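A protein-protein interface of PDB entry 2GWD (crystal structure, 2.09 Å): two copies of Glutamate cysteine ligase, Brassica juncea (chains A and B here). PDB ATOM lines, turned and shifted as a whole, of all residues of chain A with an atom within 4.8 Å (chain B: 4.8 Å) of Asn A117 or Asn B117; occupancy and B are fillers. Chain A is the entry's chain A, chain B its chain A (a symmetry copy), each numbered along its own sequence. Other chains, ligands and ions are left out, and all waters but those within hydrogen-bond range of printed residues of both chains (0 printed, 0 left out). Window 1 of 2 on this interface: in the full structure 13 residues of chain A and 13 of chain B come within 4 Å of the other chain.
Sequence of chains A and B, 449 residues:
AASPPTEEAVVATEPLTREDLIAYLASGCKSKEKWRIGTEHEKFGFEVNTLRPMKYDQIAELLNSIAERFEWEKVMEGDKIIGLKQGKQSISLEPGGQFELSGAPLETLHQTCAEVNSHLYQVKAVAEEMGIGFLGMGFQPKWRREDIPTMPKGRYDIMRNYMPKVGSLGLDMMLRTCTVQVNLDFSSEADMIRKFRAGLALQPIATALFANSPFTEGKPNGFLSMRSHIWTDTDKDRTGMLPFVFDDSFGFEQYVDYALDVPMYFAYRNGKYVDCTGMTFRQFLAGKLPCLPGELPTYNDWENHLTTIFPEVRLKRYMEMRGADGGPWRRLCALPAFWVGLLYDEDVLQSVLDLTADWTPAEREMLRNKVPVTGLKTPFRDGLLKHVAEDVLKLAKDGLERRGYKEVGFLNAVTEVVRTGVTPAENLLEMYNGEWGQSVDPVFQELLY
OH of Tyr B121 lies close to SG of Cys A113, 3.2 Å away.
The side-chain sulfur of Cys B113 sits close to the side-chain hydroxyl of Tyr A121, at 3.2 Å.
The side-chain amide oxygen of Asn B117 lies close to the side-chain amide oxygen of Asn A117 (2.9 Å).
Among the printed residues, pairs that only touch across the chains: Ala A114 with Tyr B121, Asn A117 with Tyr B121, Tyr A121 with Ala B114 and Tyr A121 with Asn B117.
Asn A117 touches two residues of chain B.
Of the printed residues of chain A, Asn B117 touches Asn A117 and Tyr A121.
Printed residues of chain A within 4 Å of Cys B113: Tyr A121 (3.1 Å).
Of the printed residues of chain B, Ala A114 touches Tyr B121 (3.5 Å).
Val A116 touches none of the printed residues of chain B.
Ser A118 touches none of the printed residues of chain B.
The nearest printed residue of chain B that does not touch Asn A117 is Ser B118 (5.0 Å).
Hydrophobic or aromatic side chains of chain A within 4 Å of the printed part of chain B: Ala A114 and Tyr A121.
Cys A113 touches Tyr B121, and with the chains exchanged Tyr A121 touches Cys B113.
Ala A114 touches Tyr B121, and with the chains exchanged Tyr A121 touches Ala B114.
Asn A117 touches its own counterpart, Asn B117.
Asn A117 touches Tyr B121, and with the chains exchanged Tyr A121 touches Asn B117.
Of the 7 pairs that touch across the chains among the printed residues, 7 have their exchanged pair printed and touching as well.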
ATOM      1  N   CYS A 113      12.521  39.140  -5.801  1.00  0.00           N
ATOM      2  CA  CYS A 113      13.253  37.899  -5.697  1.00  0.00           C
ATOM      3  C   CYS A 113      12.438  36.681  -6.176  1.00  0.00           C
ATOM      4  O   CYS A 113      12.997  35.765  -6.778  1.00  0.00           O
ATOM      5  CB  CYS A 113      13.782  37.706  -4.274  1.00  0.00           C
ATOM      6  SG  CYS A 113      15.277  36.647  -4.241  1.00  0.00           S
ATOM      7  N   ALA A 114      11.136  36.673  -5.882  1.00  0.00           N
ATOM      8  CA  ALA A 114      10.203  35.743  -6.482  1.00  0.00           C
ATOM      9  C   ALA A 114      10.246  35.822  -8.007  1.00  0.00           C
ATOM     10  O   ALA A 114      10.220  34.815  -8.681  1.00  0.00           O
ATOM     11  CB  ALA A 114       8.791  36.018  -5.983  1.00  0.00           C
ATOM     12  N   GLU A 115      10.318  37.033  -8.550  1.00  0.00           N
ATOM     13  CA  GLU A 115      10.412  37.196  -9.994  1.00  0.00           C
ATOM     14  C   GLU A 115      11.722  36.615 -10.534  1.00  0.00           C
ATOM     15  O   GLU A 115      11.738  35.997 -11.575  1.00  0.00           O
ATOM     16  CB  GLU A 115      10.311  38.673 -10.359  1.00  0.00           C
ATOM     17  CG  GLU A 115      10.207  38.933 -11.833  1.00  0.00           C
ATOM     18  CD  GLU A 115      10.295  40.407 -12.129  1.00  0.00           C
ATOM     19  OE1 GLU A 115      11.360  41.012 -11.843  1.00  0.00           O
ATOM     20  OE2 GLU A 115       9.303  40.948 -12.634  1.00  0.00           O
ATOM     21  N   VAL A 116      12.830  36.831  -9.830  1.00  0.00           N
ATOM     22  CA  VAL A 116      14.119  36.280 -10.264  1.00  0.00           C
ATOM     23  C   VAL A 116      14.009  34.737 -10.273  1.00  0.00           C
ATOM     24  O   VAL A 116      14.350  34.094 -11.252  1.00  0.00           O
ATOM     25  CB  VAL A 116      15.272  36.792  -9.368  1.00  0.00           C
ATOM     26  CG1 VAL A 116      16.563  35.970  -9.557  1.00  0.00           C
ATOM     27  CG2 VAL A 116      15.551  38.261  -9.654  1.00  0.00           C
ATOM     28  N   ASN A 117      13.465  34.161  -9.206  1.00  0.00           N
ATOM     29  CA  ASN A 117      13.332  32.715  -9.091  1.00  0.00           C
ATOM     30  C   ASN A 117      12.463  32.102 -10.194  1.00  0.00           C
ATOM     31  O   ASN A 117      12.798  31.062 -10.768  1.00  0.00           O
ATOM     32  CB  ASN A 117      12.790  32.328  -7.719  1.00  0.00           C
ATOM     33  CG  ASN A 117      12.489  30.869  -7.628  1.00  0.00           C
ATOM     34  OD1 ASN A 117      11.352  30.447  -7.864  1.00  0.00           O
ATOM     35  ND2 ASN A 117      13.512  30.068  -7.318  1.00  0.00           N
ATOM     36  N   SER A 118      11.336  32.745 -10.463  1.00  0.00           N
ATOM     37  CA  SER A 118      10.453  32.315 -11.518  1.00  0.00           C
ATOM     38  C   SER A 118      11.226  32.207 -12.820  1.00  0.00           C
ATOM     39  O   SER A 118      11.110  31.220 -13.544  1.00  0.00           O
ATOM     40  CB  SER A 118       9.329  33.329 -11.695  1.00  0.00           C
ATOM     41  OG  SER A 118       8.461  32.929 -12.723  1.00  0.00           O
ATOM     42  N   HIS A 119      12.015  33.239 -13.121  1.00  0.00           N
ATOM     43  CA  HIS A 119      12.731  33.288 -14.372  1.00  0.00           C
ATOM     44  C   HIS A 119      13.765  32.173 -14.435  1.00  0.00           C
ATOM     45  O   HIS A 119      13.861  31.458 -15.451  1.00  0.00           O
ATOM     46  CB  HIS A 119      13.383  34.649 -14.582  1.00  0.00           C
ATOM     47  CG  HIS A 119      14.252  34.722 -15.794  1.00  0.00           C
ATOM     48  ND1 HIS A 119      13.760  34.561 -17.069  1.00  0.00           N
ATOM     49  CD2 HIS A 119      15.583  34.943 -15.928  1.00  0.00           C
ATOM     50  CE1 HIS A 119      14.751  34.674 -17.934  1.00  0.00           C
ATOM     51  NE2 HIS A 119      15.872  34.889 -17.268  1.00  0.00           N
ATOM     52  N   LEU A 120      14.531  32.022 -13.353  1.00  0.00           N
ATOM     53  CA  LEU A 120      15.603  31.007 -13.305  1.00  0.00           C
ATOM     54  C   LEU A 120      15.012  29.615 -13.441  1.00  0.00           C
ATOM     55  O   LEU A 120      15.560  28.775 -14.146  1.00  0.00           O
ATOM     56  CB  LEU A 120      16.455  31.139 -12.017  1.00  0.00           C
ATOM     57  CG  LEU A 120      17.241  32.452 -11.934  1.00  0.00           C
ATOM     58  CD1 LEU A 120      17.954  32.543 -10.608  1.00  0.00           C
ATOM     59  CD2 LEU A 120      18.249  32.535 -13.086  1.00  0.00           C
ATOM     60  N   TYR A 121      13.880  29.386 -12.770  1.00  0.00           N
ATOM     61  CA  TYR A 121      13.159  28.149 -12.919  1.00  0.00           C
ATOM     62  C   TYR A 121      12.779  27.901 -14.393  1.00  0.00           C
ATOM     63  O   TYR A 121      12.990  26.814 -14.893  1.00  0.00           O
ATOM     64  CB  TYR A 121      11.891  28.081 -12.045  1.00  0.00           C
ATOM     65  CG  TYR A 121      11.121  26.846 -12.403  1.00  0.00           C
ATOM     66  CD1 TYR A 121      11.552  25.592 -11.965  1.00  0.00           C
ATOM     67  CD2 TYR A 121      10.036  26.897 -13.273  1.00  0.00           C
ATOM     68  CE1 TYR A 121      10.891  24.448 -12.321  1.00  0.00           C
ATOM     69  CE2 TYR A 121       9.375  25.741 -13.642  1.00  0.00           C
ATOM     70  CZ  TYR A 121       9.822  24.518 -13.158  1.00  0.00           C
ATOM     71  OH  TYR A 121       9.205  23.348 -13.529  1.00  0.00           O
ATOM     72  N   CYS B 113       4.587  22.062 -12.572  1.00  0.00           N
ATOM     73  CA  CYS B 113       5.910  22.077 -11.994  1.00  0.00           C
ATOM     74  C   CYS B 113       6.388  23.496 -11.627  1.00  0.00           C
ATOM     75  O   CYS B 113       7.063  23.676 -10.615  1.00  0.00           O
ATOM     76  CB  CYS B 113       6.904  21.362 -12.910  1.00  0.00           C
ATOM     77  SG  CYS B 113       8.326  20.681 -11.975  1.00  0.00           S
ATOM     78  N   ALA B 114       6.053  24.480 -12.464  1.00  0.00           N
ATOM     79  CA  ALA B 114       6.197  25.881 -12.126  1.00  0.00           C
ATOM     80  C   ALA B 114       5.458  26.216 -10.833  1.00  0.00           C
ATOM     81  O   ALA B 114       5.962  26.939 -10.001  1.00  0.00           O
ATOM     82  CB  ALA B 114       5.685  26.753 -13.264  1.00  0.00           C
ATOM     83  N   GLU B 115       4.253  25.682 -10.666  1.00  0.00           N
ATOM     84  CA  GLU B 115       3.499  25.911  -9.441  1.00  0.00           C
ATOM     85  C   GLU B 115       4.205  25.291  -8.231  1.00  0.00           C
ATOM     86  O   GLU B 115       4.242  25.878  -7.173  1.00  0.00           O
ATOM     87  CB  GLU B 115       2.097  25.331  -9.575  1.00  0.00           C
ATOM     88  CG  GLU B 115       1.179  25.681  -8.441  1.00  0.00           C
ATOM     89  CD  GLU B 115      -0.122  24.930  -8.548  1.00  0.00           C
ATOM     90  OE1 GLU B 115      -0.097  23.675  -8.471  1.00  0.00           O
ATOM     91  OE2 GLU B 115      -1.153  25.595  -8.715  1.00  0.00           O
ATOM     92  N   VAL B 116       4.752  24.088  -8.386  1.00  0.00           N
ATOM     93  CA  VAL B 116       5.474  23.440  -7.285  1.00  0.00           C
ATOM     94  C   VAL B 116       6.684  24.327  -6.909  1.00  0.00           C
ATOM     95  O   VAL B 116       6.888  24.645  -5.750  1.00  0.00           O
ATOM     96  CB  VAL B 116       5.883  21.996  -7.661  1.00  0.00           C
ATOM     97  CG1 VAL B 116       6.936  21.421  -6.693  1.00  0.00           C
ATOM     98  CG2 VAL B 116       4.660  21.090  -7.689  1.00  0.00           C
ATOM     99  N   ASN B 117       7.438  24.777  -7.907  1.00  0.00           N
ATOM    100  CA  ASN B 117       8.618  25.599  -7.674  1.00  0.00           C
ATOM    101  C   ASN B 117       8.301  26.920  -6.965  1.00  0.00           C
ATOM    102  O   ASN B 117       9.009  27.338  -6.045  1.00  0.00           O
ATOM    103  CB  ASN B 117       9.357  25.868  -8.980  1.00  0.00           C
ATOM    104  CG  ASN B 117      10.476  26.841  -8.800  1.00  0.00           C
ATOM    105  OD1 ASN B 117      10.298  28.046  -9.001  1.00  0.00           O
ATOM    106  ND2 ASN B 117      11.642  26.337  -8.383  1.00  0.00           N
ATOM    107  N   SER B 118       7.245  27.579  -7.420  1.00  0.00           N
ATOM    108  CA  SER B 118       6.795  28.803  -6.808  1.00  0.00           C
ATOM    109  C   SER B 118       6.574  28.582  -5.323  1.00  0.00           C
ATOM    110  O   SER B 118       7.008  29.379  -4.495  1.00  0.00           O
ATOM    111  CB  SER B 118       5.481  29.244  -7.441  1.00  0.00           C
ATOM    112  OG  SER B 118       5.023  30.434  -6.854  1.00  0.00           O
ATOM    113  N   HIS B 119       5.886  27.490  -4.989  1.00  0.00           N
ATOM    114  CA  HIS B 119       5.540  27.220  -3.614  1.00  0.00           C
ATOM    115  C   HIS B 119       6.796  26.970  -2.792  1.00  0.00           C
ATOM    116  O   HIS B 119       6.952  27.535  -1.692  1.00  0.00           O
ATOM    117  CB  HIS B 119       4.576  26.046  -3.509  1.00  0.00           C
ATOM    118  CG  HIS B 119       4.284  25.629  -2.105  1.00  0.00           C
ATOM    119  ND1 HIS B 119       3.657  26.456  -1.202  1.00  0.00           N
ATOM    120  CD2 HIS B 119       4.528  24.468  -1.448  1.00  0.00           C
ATOM    121  CE1 HIS B 119       3.535  25.825  -0.048  1.00  0.00           C
ATOM    122  NE2 HIS B 119       4.070  24.623  -0.163  1.00  0.00           N
ATOM    123  N   LEU B 120       7.688  26.132  -3.323  1.00  0.00           N
ATOM    124  CA  LEU B 120       8.926  25.770  -2.604  1.00  0.00           C
ATOM    125  C   LEU B 120       9.781  27.004  -2.381  1.00  0.00           C
ATOM    126  O   LEU B 120      10.345  27.182  -1.306  1.00  0.00           O
ATOM    127  CB  LEU B 120       9.713  24.660  -3.347  1.00  0.00           C
ATOM    128  CG  LEU B 120       8.969  23.323  -3.416  1.00  0.00           C
ATOM    129  CD1 LEU B 120       9.756  22.338  -4.244  1.00  0.00           C
ATOM    130  CD2 LEU B 120       8.747  22.771  -2.003  1.00  0.00           C
ATOM    131  N   TYR B 121       9.859  27.862  -3.401  1.00  0.00           N
ATOM    132  CA  TYR B 121      10.536  29.126  -3.267  1.00  0.00           C
ATOM    133  C   TYR B 121       9.931  29.961  -2.119  1.00  0.00           C
ATOM    134  O   TYR B 121      10.665  30.484  -1.305  1.00  0.00           O
ATOM    135  CB  TYR B 121      10.525  29.956  -4.565  1.00  0.00           C
ATOM    136  CG  TYR B 121      11.086  31.315  -4.277  1.00  0.00           C
ATOM    137  CD1 TYR B 121      12.462  31.491  -4.114  1.00  0.00           C
ATOM    138  CD2 TYR B 121      10.255  32.407  -4.043  1.00  0.00           C
ATOM    139  CE1 TYR B 121      12.991  32.715  -3.802  1.00  0.00           C
ATOM    140  CE2 TYR B 121      10.788  33.639  -3.717  1.00  0.00           C
ATOM    141  CZ  TYR B 121      12.165  33.775  -3.595  1.00  0.00           C
ATOM    142  OH  TYR B 121      12.724  34.979  -3.243  1.00  0.00           O
